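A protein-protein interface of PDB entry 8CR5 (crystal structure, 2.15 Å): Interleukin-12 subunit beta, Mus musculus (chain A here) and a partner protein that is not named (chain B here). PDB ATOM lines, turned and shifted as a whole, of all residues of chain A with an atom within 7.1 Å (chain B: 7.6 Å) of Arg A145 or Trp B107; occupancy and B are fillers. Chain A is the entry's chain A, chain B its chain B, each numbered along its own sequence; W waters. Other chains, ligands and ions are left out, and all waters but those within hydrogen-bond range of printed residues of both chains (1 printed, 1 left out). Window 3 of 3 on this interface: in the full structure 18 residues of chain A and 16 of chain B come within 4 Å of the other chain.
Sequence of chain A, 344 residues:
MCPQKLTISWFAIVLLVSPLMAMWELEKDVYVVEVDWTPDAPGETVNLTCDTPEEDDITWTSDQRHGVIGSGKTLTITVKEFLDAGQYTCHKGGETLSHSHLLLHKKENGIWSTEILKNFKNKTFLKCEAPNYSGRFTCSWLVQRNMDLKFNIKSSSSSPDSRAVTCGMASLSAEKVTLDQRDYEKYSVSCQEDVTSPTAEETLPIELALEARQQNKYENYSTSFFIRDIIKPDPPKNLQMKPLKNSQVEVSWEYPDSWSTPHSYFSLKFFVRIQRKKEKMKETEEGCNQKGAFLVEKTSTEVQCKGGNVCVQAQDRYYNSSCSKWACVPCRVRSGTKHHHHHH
The side-chain amide oxygen of Gln A215 sits close to the side-chain amide oxygen of Gln B109.
The side-chain carboxylate (OE2) of Glu B108 is in salt-bridge range of the side-chain amino group (NZ) of Lys A217 (3.1 Å).
NE2 of Gln B109 lies within hydrogen-bond range of O of Gln A214 (3.1 Å).
Hydrophobic or aromatic side chains of chain B within 4 Å of the printed part of chain A: Trp B107.
Along chain B the printed residues that touch a printed residue of chain A span positions 56 to 109.
Printed residues of chain A that touch a printed residue of chain B: Glu A115, Arg A145, Gln A214, Gln A215 and Lys A217.
Among the printed residues, 10 pairs touch across the chains.
O of Thr B57 lies within hydrogen-bond range of N of Glu B108 (2.9 Å).
The side-chain hydroxyl (OG1) of Thr B57 sits at hydrogen-bond distance from the side-chain carboxylate (OD1) of Asp B58 (2.7 Å).
The side-chain amide oxygen of Gln A214 sits close to the backbone carbonyl oxygen of Arg A145.
The side-chain carboxylate (OD2) of Asp B110 is in hydrogen-bond range of the backbone NH (N) of Trp B107, at 3.1 Å.
OE1 of Glu A115 lies within salt-bridge range of NZ of Lys A217, at 2.9 Å.
OG of Ser B55 sits close to N of Thr B57 (3.2 Å).
Water W1 lies within hydrogen-bond range of OE2 of Glu B108 (2.5 Å), NE2 of Gln B109 (3.1 Å) and NZ of Lys A217 (3.5 Å).
Among the printed residues, merely in contact across the chains: Glu A115 with Lys B56 (2.9 Å), Glu A115 with Thr B57 (3.6 Å), Arg A145 with Trp B107 (3.5 Å), Gln A214 with Trp B107 (3.5 Å), Gln A215 with Trp B107 (3.96 Å), Lys A217 with Thr B57 (3.4 Å) and Lys A217 with Gln B109 (3.5 Å).
Of chain B, only Trp B107 comes within 4 Å of Arg A145.
Of chain A, only Arg A145, Gln A214 and Gln A215 come within 4 Å of Trp B107.
Of the printed residues of chain A, Glu B108 touches Lys A217 (3.1 Å).
Of the printed residues of chain B, Lys A217 touches Thr B57 (3.4 Å), Glu B108 (3.1 Å) and Gln B109 (3.5 Å).
Of the printed residues of chain B, Glu A115 touches Lys B56 and Thr B57.
Printed residues of chain A within 4 Å of Gln B109: Gln A214 (3.1 Å), Gln A215 (3.2 Å) and Lys A217 (3.5 Å).
Printed residues of chain A within 4 Å of Thr B57: Glu A115 and Lys A217.
Leu A149 touches none of the printed residues of chain B.
Gly B111 touches none of the printed residues of chain A.
The nearest residue of chain B that does not touch Arg A145 is Asp B110 (5.9 Å).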
ATOM      1  N   GLU A 115      -4.223  -6.967   6.504  1.00  0.00           N
ATOM      2  CA  GLU A 115      -4.728  -8.312   6.755  1.00  0.00           C
ATOM      3  C   GLU A 115      -6.173  -8.544   6.349  1.00  0.00           C
ATOM      4  O   GLU A 115      -6.569  -9.706   6.210  1.00  0.00           O
ATOM      5  CB  GLU A 115      -4.582  -8.676   8.239  1.00  0.00           C
ATOM      6  CG  GLU A 115      -3.167  -8.998   8.586  1.00  0.00           C
ATOM      7  CD  GLU A 115      -2.693  -8.164   9.771  1.00  0.00           C
ATOM      8  OE1 GLU A 115      -3.559  -7.521  10.382  1.00  0.00           O
ATOM      9  OE2 GLU A 115      -1.495  -8.191  10.047  1.00  0.00           O
ATOM     10  N   ILE A 116      -6.978  -7.496   6.192  1.00  0.00           N
ATOM     11  CA  ILE A 116      -8.345  -7.704   5.723  1.00  0.00           C
ATOM     12  C   ILE A 116      -8.331  -8.272   4.310  1.00  0.00           C
ATOM     13  O   ILE A 116      -9.077  -9.207   3.991  1.00  0.00           O
ATOM     14  CB  ILE A 116      -9.150  -6.395   5.798  1.00  0.00           C
ATOM     15  CG1 ILE A 116      -9.192  -5.881   7.236  1.00  0.00           C
ATOM     16  CG2 ILE A 116     -10.565  -6.608   5.275  1.00  0.00           C
ATOM     17  CD1 ILE A 116      -9.634  -4.439   7.349  1.00  0.00           C
ATOM     18  N   VAL A 143     -10.870 -10.858  -0.255  1.00  0.00           N
ATOM     19  CA  VAL A 143     -10.969 -11.014   1.190  1.00  0.00           C
ATOM     20  C   VAL A 143     -11.494 -12.413   1.479  1.00  0.00           C
ATOM     21  O   VAL A 143     -12.201 -13.014   0.664  1.00  0.00           O
ATOM     22  CB  VAL A 143     -11.874  -9.948   1.849  1.00  0.00           C
ATOM     23  CG1 VAL A 143     -11.482  -8.546   1.406  1.00  0.00           C
ATOM     24  CG2 VAL A 143     -13.321 -10.224   1.542  1.00  0.00           C
ATOM     25  N   GLN A 144     -11.135 -12.933   2.648  1.00  0.00           N
ATOM     26  CA  GLN A 144     -11.544 -14.270   3.064  1.00  0.00           C
ATOM     27  C   GLN A 144     -12.606 -14.264   4.151  1.00  0.00           C
ATOM     28  O   GLN A 144     -13.541 -15.066   4.095  1.00  0.00           O
ATOM     29  CB  GLN A 144     -10.325 -15.065   3.547  1.00  0.00           C
ATOM     30  CG  GLN A 144     -10.565 -16.558   3.656  1.00  0.00           C
ATOM     31  CD  GLN A 144     -10.001 -17.139   4.934  1.00  0.00           C
ATOM     32  OE1 GLN A 144      -8.806 -17.416   5.028  1.00  0.00           O
ATOM     33  NE2 GLN A 144     -10.861 -17.324   5.929  1.00  0.00           N
ATOM     34  N   ARG A 145     -12.493 -13.378   5.139  1.00  0.00           N
ATOM     35  CA  ARG A 145     -13.514 -13.236   6.176  1.00  0.00           C
ATOM     36  C   ARG A 145     -14.514 -12.186   5.710  1.00  0.00           C
ATOM     37  O   ARG A 145     -14.273 -10.981   5.829  1.00  0.00           O
ATOM     38  CB  ARG A 145     -12.889 -12.864   7.514  1.00  0.00           C
ATOM     39  CG  ARG A 145     -13.895 -12.849   8.646  1.00  0.00           C
ATOM     40  CD  ARG A 145     -13.232 -12.749  10.005  1.00  0.00           C
ATOM     41  NE  ARG A 145     -14.226 -12.563  11.056  1.00  0.00           N
ATOM     42  CZ  ARG A 145     -14.532 -13.478  11.965  1.00  0.00           C
ATOM     43  NH1 ARG A 145     -13.930 -14.656  11.991  1.00  0.00           N
ATOM     44  NH2 ARG A 145     -15.469 -13.205  12.869  1.00  0.00           N
ATOM     45  N   ASN A 146     -15.649 -12.644   5.194  1.00  0.00           N
ATOM     46  CA  ASN A 146     -16.618 -11.775   4.527  1.00  0.00           C
ATOM     47  C   ASN A 146     -17.774 -11.419   5.457  1.00  0.00           C
ATOM     48  O   ASN A 146     -18.937 -11.721   5.191  1.00  0.00           O
ATOM     49  CB  ASN A 146     -17.126 -12.446   3.258  1.00  0.00           C
ATOM     50  CG  ASN A 146     -16.138 -12.358   2.124  1.00  0.00           C
ATOM     51  OD1 ASN A 146     -16.164 -11.412   1.340  1.00  0.00           O
ATOM     52  ND2 ASN A 146     -15.249 -13.340   2.035  1.00  0.00           N
ATOM     53  N   MET A 147     -17.432 -10.758   6.562  1.00  0.00           N
ATOM     54  CA  MET A 147     -18.407 -10.329   7.557  1.00  0.00           C
ATOM     55  C   MET A 147     -18.027  -8.941   8.052  1.00  0.00           C
ATOM     56  O   MET A 147     -16.843  -8.659   8.259  1.00  0.00           O
ATOM     57  CB  MET A 147     -18.473 -11.299   8.751  1.00  0.00           C
ATOM     58  CG  MET A 147     -18.518 -12.791   8.408  1.00  0.00           C
ATOM     59  SD  MET A 147     -19.977 -13.357   7.508  1.00  0.00           S
ATOM     60  CE  MET A 147     -21.258 -12.414   8.307  1.00  0.00           C
ATOM     61  N   ASP A 148     -19.032  -8.081   8.245  1.00  0.00           N
ATOM     62  CA  ASP A 148     -18.830  -6.745   8.819  1.00  0.00           C
ATOM     63  C   ASP A 148     -17.855  -5.910   7.988  1.00  0.00           C
ATOM     64  O   ASP A 148     -17.041  -5.156   8.523  1.00  0.00           O
ATOM     65  CB  ASP A 148     -18.359  -6.840  10.272  1.00  0.00           C
ATOM     66  CG  ASP A 148     -19.361  -7.547  11.162  1.00  0.00           C
ATOM     67  OD1 ASP A 148     -20.031  -8.485  10.678  1.00  0.00           O
ATOM     68  OD2 ASP A 148     -19.455  -7.192  12.353  1.00  0.00           O
ATOM     69  N   LEU A 149     -17.941  -6.037   6.668  1.00  0.00           N
ATOM     70  CA  LEU A 149     -17.035  -5.337   5.770  1.00  0.00           C
ATOM     71  C   LEU A 149     -17.632  -4.020   5.284  1.00  0.00           C
ATOM     72  O   LEU A 149     -18.849  -3.878   5.137  1.00  0.00           O
ATOM     73  CB  LEU A 149     -16.679  -6.216   4.570  1.00  0.00           C
ATOM     74  CG  LEU A 149     -15.814  -7.442   4.861  1.00  0.00           C
ATOM     75  CD1 LEU A 149     -15.434  -8.140   3.574  1.00  0.00           C
ATOM     76  CD2 LEU A 149     -14.565  -7.020   5.622  1.00  0.00           C
ATOM     77  N   ASP A 183     -11.136 -20.645  -0.428  1.00  0.00           N
ATOM     78  CA  ASP A 183     -12.195 -19.824  -0.993  1.00  0.00           C
ATOM     79  C   ASP A 183     -12.035 -18.367  -0.580  1.00  0.00           C
ATOM     80  O   ASP A 183     -11.699 -18.063   0.569  1.00  0.00           O
ATOM     81  CB  ASP A 183     -13.566 -20.342  -0.561  1.00  0.00           C
ATOM     82  CG  ASP A 183     -13.885 -21.699  -1.154  1.00  0.00           C
ATOM     83  OD1 ASP A 183     -13.886 -21.819  -2.398  1.00  0.00           O
ATOM     84  OD2 ASP A 183     -14.134 -22.645  -0.378  1.00  0.00           O
ATOM     85  N   TYR A 184     -12.274 -17.471  -1.534  1.00  0.00           N
ATOM     86  CA  TYR A 184     -12.233 -16.037  -1.297  1.00  0.00           C
ATOM     87  C   TYR A 184     -13.364 -15.387  -2.078  1.00  0.00           C
ATOM     88  O   TYR A 184     -13.942 -15.984  -2.987  1.00  0.00           O
ATOM     89  CB  TYR A 184     -10.889 -15.421  -1.714  1.00  0.00           C
ATOM     90  CG  TYR A 184      -9.680 -16.049  -1.058  1.00  0.00           C
ATOM     91  CD1 TYR A 184      -9.095 -17.193  -1.583  1.00  0.00           C
ATOM     92  CD2 TYR A 184      -9.117 -15.489   0.080  1.00  0.00           C
ATOM     93  CE1 TYR A 184      -7.990 -17.768  -0.988  1.00  0.00           C
ATOM     94  CE2 TYR A 184      -8.011 -16.056   0.682  1.00  0.00           C
ATOM     95  CZ  TYR A 184      -7.451 -17.195   0.144  1.00  0.00           C
ATOM     96  OH  TYR A 184      -6.349 -17.764   0.739  1.00  0.00           O
ATOM     97  N   GLU A 185     -13.676 -14.149  -1.709  1.00  0.00           N
ATOM     98  CA  GLU A 185     -14.657 -13.343  -2.423  1.00  0.00           C
ATOM     99  C   GLU A 185     -13.928 -12.210  -3.128  1.00  0.00           C
ATOM    100  O   GLU A 185     -13.241 -11.411  -2.482  1.00  0.00           O
ATOM    101  CB  GLU A 185     -15.724 -12.804  -1.471  1.00  0.00           C
ATOM    102  CG  GLU A 185     -16.620 -13.885  -0.892  1.00  0.00           C
ATOM    103  CD  GLU A 185     -18.066 -13.748  -1.326  1.00  0.00           C
ATOM    104  OE1 GLU A 185     -18.432 -12.679  -1.860  1.00  0.00           O
ATOM    105  OE2 GLU A 185     -18.839 -14.709  -1.132  1.00  0.00           O
ATOM    106  N   TYR A 187     -14.114  -8.881  -4.842  1.00  0.00           N
ATOM    107  CA  TYR A 187     -14.900  -7.680  -5.072  1.00  0.00           C
ATOM    108  C   TYR A 187     -14.386  -6.953  -6.306  1.00  0.00           C
ATOM    109  O   TYR A 187     -13.209  -7.043  -6.657  1.00  0.00           O
ATOM    110  CB  TYR A 187     -14.838  -6.752  -3.857  1.00  0.00           C
ATOM    111  CG  TYR A 187     -15.474  -7.331  -2.617  1.00  0.00           C
ATOM    112  CD1 TYR A 187     -14.802  -8.267  -1.844  1.00  0.00           C
ATOM    113  CD2 TYR A 187     -16.748  -6.948  -2.221  1.00  0.00           C
ATOM    114  CE1 TYR A 187     -15.378  -8.801  -0.716  1.00  0.00           C
ATOM    115  CE2 TYR A 187     -17.332  -7.478  -1.089  1.00  0.00           C
ATOM    116  CZ  TYR A 187     -16.641  -8.405  -0.339  1.00  0.00           C
ATOM    117  OH  TYR A 187     -17.212  -8.941   0.790  1.00  0.00           O
ATOM    118  N   GLN A 214     -13.282  -3.748   8.741  1.00  0.00           N
ATOM    119  CA  GLN A 214     -13.775  -5.056   9.165  1.00  0.00           C
ATOM    120  C   GLN A 214     -14.079  -4.978  10.655  1.00  0.00           C
ATOM    121  O   GLN A 214     -13.157  -4.945  11.478  1.00  0.00           O
ATOM    122  CB  GLN A 214     -12.765  -6.164   8.871  1.00  0.00           C
ATOM    123  CG  GLN A 214     -13.337  -7.564   9.036  1.00  0.00           C
ATOM    124  CD  GLN A 214     -12.355  -8.648   8.639  1.00  0.00           C
ATOM    125  OE1 GLN A 214     -12.659  -9.506   7.810  1.00  0.00           O
ATOM    126  NE2 GLN A 214     -11.169  -8.619   9.235  1.00  0.00           N
ATOM    127  N   GLN A 215     -15.370  -4.960  10.993  1.00  0.00           N
ATOM    128  CA  GLN A 215     -15.841  -4.742  12.358  1.00  0.00           C
ATOM    129  C   GLN A 215     -15.288  -3.435  12.914  1.00  0.00           C
ATOM    130  O   GLN A 215     -15.780  -2.357  12.572  1.00  0.00           O
ATOM    131  CB  GLN A 215     -15.464  -5.912  13.269  1.00  0.00           C
ATOM    132  CG  GLN A 215     -16.350  -6.040  14.498  1.00  0.00           C
ATOM    133  CD  GLN A 215     -16.056  -7.288  15.309  1.00  0.00           C
ATOM    134  OE1 GLN A 215     -15.337  -8.180  14.860  1.00  0.00           O
ATOM    135  NE2 GLN A 215     -16.612  -7.355  16.512  1.00  0.00           N
ATOM    136  N   LYS A 217     -11.872  -2.689  12.757  1.00  0.00           N
ATOM    137  CA  LYS A 217     -10.534  -2.567  12.203  1.00  0.00           C
ATOM    138  C   LYS A 217     -10.570  -1.699  10.953  1.00  0.00           C
ATOM    139  O   LYS A 217     -11.469  -1.838  10.117  1.00  0.00           O
ATOM    140  CB  LYS A 217      -9.974  -3.950  11.866  1.00  0.00           C
ATOM    141  CG  LYS A 217      -8.481  -4.018  11.641  1.00  0.00           C
ATOM    142  CD  LYS A 217      -8.136  -5.389  11.089  1.00  0.00           C
ATOM    143  CE  LYS A 217      -6.671  -5.720  11.240  1.00  0.00           C
ATOM    144  NZ  LYS A 217      -6.432  -7.141  10.864  1.00  0.00           N
ATOM    145  N   SER B  55      -1.359 -16.449  13.361  1.00  0.00           N
ATOM    146  CA  SER B  55      -1.302 -15.573  12.202  1.00  0.00           C
ATOM    147  C   SER B  55      -1.195 -14.148  12.720  1.00  0.00           C
ATOM    148  O   SER B  55      -1.023 -13.919  13.918  1.00  0.00           O
ATOM    149  CB  SER B  55      -2.526 -15.764  11.295  1.00  0.00           C
ATOM    150  OG  SER B  55      -3.655 -15.089  11.818  1.00  0.00           O
ATOM    151  N   LYS B  56      -1.310 -13.182  11.817  1.00  0.00           N
ATOM    152  CA  LYS B  56      -1.253 -11.793  12.246  1.00  0.00           C
ATOM    153  C   LYS B  56      -2.456 -11.418  13.106  1.00  0.00           C
ATOM    154  O   LYS B  56      -2.354 -10.523  13.953  1.00  0.00           O
ATOM    155  CB  LYS B  56      -1.156 -10.885  11.026  1.00  0.00           C
ATOM    156  CG  LYS B  56       0.188 -10.923  10.303  1.00  0.00           C
ATOM    157  CD  LYS B  56       1.309 -10.373  11.172  1.00  0.00           C
ATOM    158  CE  LYS B  56       2.424  -9.766  10.329  1.00  0.00           C
ATOM    159  NZ  LYS B  56       2.859  -8.436  10.846  1.00  0.00           N
ATOM    160  N   THR B  57      -3.592 -12.096  12.918  1.00  0.00           N
ATOM    161  CA  THR B  57      -4.817 -11.781  13.641  1.00  0.00           C
ATOM    162  C   THR B  57      -5.361 -12.921  14.488  1.00  0.00           C
ATOM    163  O   THR B  57      -6.168 -12.659  15.386  1.00  0.00           O
ATOM    164  CB  THR B  57      -5.925 -11.348  12.666  1.00  0.00           C
ATOM    165  OG1 THR B  57      -6.336 -12.475  11.883  1.00  0.00           O
ATOM    166  CG2 THR B  57      -5.431 -10.248  11.740  1.00  0.00           C
ATOM    167  N   ASP B  58      -4.962 -14.163  14.231  1.00  0.00           N
ATOM    168  CA  ASP B  58      -5.566 -15.325  14.866  1.00  0.00           C
ATOM    169  C   ASP B  58      -4.677 -15.866  15.980  1.00  0.00           C
ATOM    170  O   ASP B  58      -3.453 -15.718  15.952  1.00  0.00           O
ATOM    171  CB  ASP B  58      -5.830 -16.424  13.835  1.00  0.00           C
ATOM    172  CG  ASP B  58      -6.921 -16.050  12.852  1.00  0.00           C
ATOM    173  OD1 ASP B  58      -7.231 -14.845  12.734  1.00  0.00           O
ATOM    174  OD2 ASP B  58      -7.467 -16.960  12.195  1.00  0.00           O
ATOM    175  N   TYR B  59      -5.313 -16.495  16.966  1.00  0.00           N
ATOM    176  CA  TYR B  59      -4.631 -17.057  18.122  1.00  0.00           C
ATOM    177  C   TYR B  59      -5.185 -18.446  18.409  1.00  0.00           C
ATOM    178  O   TYR B  59      -6.224 -18.848  17.875  1.00  0.00           O
ATOM    179  CB  TYR B  59      -4.782 -16.150  19.352  1.00  0.00           C
ATOM    180  CG  TYR B  59      -4.132 -14.795  19.189  1.00  0.00           C
ATOM    181  CD1 TYR B  59      -4.754 -13.786  18.463  1.00  0.00           C
ATOM    182  CD2 TYR B  59      -2.892 -14.528  19.754  1.00  0.00           C
ATOM    183  CE1 TYR B  59      -4.160 -12.550  18.305  1.00  0.00           C
ATOM    184  CE2 TYR B  59      -2.293 -13.292  19.607  1.00  0.00           C
ATOM    185  CZ  TYR B  59      -2.930 -12.309  18.879  1.00  0.00           C
ATOM    186  OH  TYR B  59      -2.338 -11.078  18.726  1.00  0.00           O
ATOM    187  N   GLU B  60      -4.486 -19.184  19.270  1.00  0.00           N
ATOM    188  CA  GLU B  60      -4.859 -20.562  19.547  1.00  0.00           C
ATOM    189  C   GLU B  60      -4.338 -20.986  20.912  1.00  0.00           C
ATOM    190  O   GLU B  60      -3.228 -20.616  21.304  1.00  0.00           O
ATOM    191  CB  GLU B  60      -4.322 -21.505  18.464  1.00  0.00           C
ATOM    192  CG  GLU B  60      -4.536 -22.982  18.755  1.00  0.00           C
ATOM    193  CD  GLU B  60      -4.288 -23.852  17.543  1.00  0.00           C
ATOM    194  OE1 GLU B  60      -5.238 -24.063  16.758  1.00  0.00           O
ATOM    195  OE2 GLU B  60      -3.143 -24.321  17.373  1.00  0.00           O
ATOM    196  N   PHE B  96     -14.542 -20.746  26.602  1.00  0.00           N
ATOM    197  CA  PHE B  96     -14.808 -21.494  25.377  1.00  0.00           C
ATOM    198  C   PHE B  96     -15.120 -22.931  25.759  1.00  0.00           C
ATOM    199  O   PHE B  96     -14.300 -23.590  26.408  1.00  0.00           O
ATOM    200  CB  PHE B  96     -13.611 -21.483  24.415  1.00  0.00           C
ATOM    201  CG  PHE B  96     -13.045 -20.120  24.123  1.00  0.00           C
ATOM    202  CD1 PHE B  96     -12.236 -19.472  25.044  1.00  0.00           C
ATOM    203  CD2 PHE B  96     -13.276 -19.512  22.899  1.00  0.00           C
ATOM    204  CE1 PHE B  96     -11.700 -18.227  24.763  1.00  0.00           C
ATOM    205  CE2 PHE B  96     -12.740 -18.273  22.611  1.00  0.00           C
ATOM    206  CZ  PHE B  96     -11.952 -17.628  23.544  1.00  0.00           C
ATOM    207  N   GLN B 105      -9.621 -21.899  18.979  1.00  0.00           N
ATOM    208  CA  GLN B 105      -9.197 -20.868  18.044  1.00  0.00           C
ATOM    209  C   GLN B 105      -9.996 -19.595  18.284  1.00  0.00           C
ATOM    210  O   GLN B 105     -11.210 -19.642  18.502  1.00  0.00           O
ATOM    211  CB  GLN B 105      -9.373 -21.336  16.596  1.00  0.00           C
ATOM    212  CG  GLN B 105      -8.451 -22.477  16.199  1.00  0.00           C
ATOM    213  CD  GLN B 105      -8.917 -23.818  16.735  1.00  0.00           C
ATOM    214  OE1 GLN B 105     -10.116 -24.060  16.877  1.00  0.00           O
ATOM    215  NE2 GLN B 105      -7.967 -24.693  17.049  1.00  0.00           N
ATOM    216  N   PHE B 106      -9.303 -18.461  18.258  1.00  0.00           N
ATOM    217  CA  PHE B 106      -9.947 -17.158  18.345  1.00  0.00           C
ATOM    218  C   PHE B 106      -9.073 -16.147  17.614  1.00  0.00           C
ATOM    219  O   PHE B 106      -8.049 -16.499  17.021  1.00  0.00           O
ATOM    220  CB  PHE B 106     -10.214 -16.758  19.805  1.00  0.00           C
ATOM    221  CG  PHE B 106      -8.970 -16.573  20.634  1.00  0.00           C
ATOM    222  CD1 PHE B 106      -8.297 -17.666  21.156  1.00  0.00           C
ATOM    223  CD2 PHE B 106      -8.493 -15.304  20.917  1.00  0.00           C
ATOM    224  CE1 PHE B 106      -7.163 -17.496  21.930  1.00  0.00           C
ATOM    225  CE2 PHE B 106      -7.362 -15.128  21.691  1.00  0.00           C
ATOM    226  CZ  PHE B 106      -6.697 -16.227  22.199  1.00  0.00           C
ATOM    227  N   TRP B 107      -9.490 -14.884  17.644  1.00  0.00           N
ATOM    228  CA  TRP B 107      -8.775 -13.851  16.911  1.00  0.00           C
ATOM    229  C   TRP B 107      -8.886 -12.528  17.658  1.00  0.00           C
ATOM    230  O   TRP B 107      -9.622 -12.401  18.641  1.00  0.00           O
ATOM    231  CB  TRP B 107      -9.280 -13.755  15.462  1.00  0.00           C
ATOM    232  CG  TRP B 107     -10.499 -12.907  15.233  1.00  0.00           C
ATOM    233  CD1 TRP B 107     -11.608 -12.819  16.026  1.00  0.00           C
ATOM    234  CD2 TRP B 107     -10.747 -12.063  14.102  1.00  0.00           C
ATOM    235  NE1 TRP B 107     -12.519 -11.953  15.470  1.00  0.00           N
ATOM    236  CE2 TRP B 107     -12.015 -11.478  14.288  1.00  0.00           C
ATOM    237  CE3 TRP B 107     -10.014 -11.738  12.957  1.00  0.00           C
ATOM    238  CZ2 TRP B 107     -12.566 -10.586  13.368  1.00  0.00           C
ATOM    239  CZ3 TRP B 107     -10.562 -10.853  12.046  1.00  0.00           C
ATOM    240  CH2 TRP B 107     -11.825 -10.286  12.258  1.00  0.00           C
ATOM    241  N   GLU B 108      -8.140 -11.538  17.163  1.00  0.00           N
ATOM    242  CA  GLU B 108      -7.888 -10.305  17.901  1.00  0.00           C
ATOM    243  C   GLU B 108      -9.150  -9.513  18.214  1.00  0.00           C
ATOM    244  O   GLU B 108      -9.122  -8.663  19.112  1.00  0.00           O
ATOM    245  CB  GLU B 108      -6.912  -9.428  17.115  1.00  0.00           C
ATOM    246  CG  GLU B 108      -7.438  -9.017  15.748  1.00  0.00           C
ATOM    247  CD  GLU B 108      -6.437  -8.202  14.953  1.00  0.00           C
ATOM    248  OE1 GLU B 108      -5.253  -8.158  15.349  1.00  0.00           O
ATOM    249  OE2 GLU B 108      -6.834  -7.610  13.928  1.00  0.00           O
ATOM    250  N   GLN B 109     -10.251  -9.751  17.501  1.00  0.00           N
ATOM    251  CA  GLN B 109     -11.492  -9.025  17.744  1.00  0.00           C
ATOM    252  C   GLN B 109     -12.532  -9.859  18.490  1.00  0.00           C
ATOM    253  O   GLN B 109     -13.715  -9.511  18.482  1.00  0.00           O
ATOM    254  CB  GLN B 109     -12.073  -8.507  16.425  1.00  0.00           C
ATOM    255  CG  GLN B 109     -11.185  -7.491  15.716  1.00  0.00           C
ATOM    256  CD  GLN B 109     -11.959  -6.588  14.768  1.00  0.00           C
ATOM    257  OE1 GLN B 109     -12.905  -5.911  15.172  1.00  0.00           O
ATOM    258  NE2 GLN B 109     -11.561  -6.578  13.501  1.00  0.00           N
ATOM    259  N   ASP B 110     -12.118 -10.943  19.146  1.00  0.00           N
ATOM    260  CA  ASP B 110     -13.055 -11.757  19.911  1.00  0.00           C
ATOM    261  C   ASP B 110     -13.290 -11.241  21.320  1.00  0.00           C
ATOM    262  O   ASP B 110     -14.171 -11.763  22.008  1.00  0.00           O
ATOM    263  CB  ASP B 110     -12.578 -13.210  19.998  1.00  0.00           C
ATOM    264  CG  ASP B 110     -13.171 -14.077  18.914  1.00  0.00           C
ATOM    265  OD1 ASP B 110     -14.358 -13.865  18.596  1.00  0.00           O
ATOM    266  OD2 ASP B 110     -12.454 -14.949  18.386  1.00  0.00           O
ATOM    267  N   GLY B 111     -12.526 -10.251  21.773  1.00  0.00           N
ATOM    268  CA  GLY B 111     -12.746  -9.649  23.074  1.00  0.00           C
ATOM    269  C   GLY B 111     -11.694  -9.953  24.119  1.00  0.00           C
ATOM    270  O   GLY B 111     -11.843  -9.506  25.263  1.00  0.00           O
ATOM    271  N   ILE B 112     -10.646 -10.688  23.778  1.00  0.00           N
ATOM    272  CA  ILE B 112      -9.570 -11.018  24.709  1.00  0.00           C
ATOM    273  C   ILE B 112      -8.375 -10.128  24.389  1.00  0.00           C
ATOM    274  O   ILE B 112      -7.961 -10.068  23.223  1.00  0.00           O
ATOM    275  CB  ILE B 112      -9.179 -12.505  24.621  1.00  0.00           C
ATOM    276  CG1 ILE B 112     -10.250 -13.381  25.276  1.00  0.00           C
ATOM    277  CG2 ILE B 112      -7.829 -12.741  25.280  1.00  0.00           C
ATOM    278  CD1 ILE B 112      -9.913 -14.857  25.272  1.00  0.00           C
ATOM    279  N   PRO B 113      -7.801  -9.432  25.371  1.00  0.00           N
ATOM    280  CA  PRO B 113      -6.655  -8.563  25.080  1.00  0.00           C
ATOM    281  C   PRO B 113      -5.432  -9.372  24.681  1.00  0.00           C
ATOM    282  O   PRO B 113      -5.164 -10.441  25.232  1.00  0.00           O
ATOM    283  CB  PRO B 113      -6.423  -7.819  26.402  1.00  0.00           C
ATOM    284  CG  PRO B 113      -7.665  -8.048  27.219  1.00  0.00           C
ATOM    285  CD  PRO B 113      -8.195  -9.376  26.787  1.00  0.00           C
ATOM    286  N   VAL B 114      -4.689  -8.849  23.707  1.00  0.00           N
ATOM    287  CA  VAL B 114      -3.442  -9.467  23.264  1.00  0.00           C
ATOM    288  C   VAL B 114      -2.218  -8.633  23.606  1.00  0.00           C
ATOM    289  O   VAL B 114      -1.090  -9.126  23.441  1.00  0.00           O
ATOM    290  CB  VAL B 114      -3.465  -9.774  21.752  1.00  0.00           C
ATOM    291  CG1 VAL B 114      -4.765 -10.467  21.369  1.00  0.00           C
ATOM    292  CG2 VAL B 114      -3.270  -8.501  20.944  1.00  0.00           C
HETATM  293  O   HOH W   1      -9.048  -8.251  12.874  1.00  0.00           O
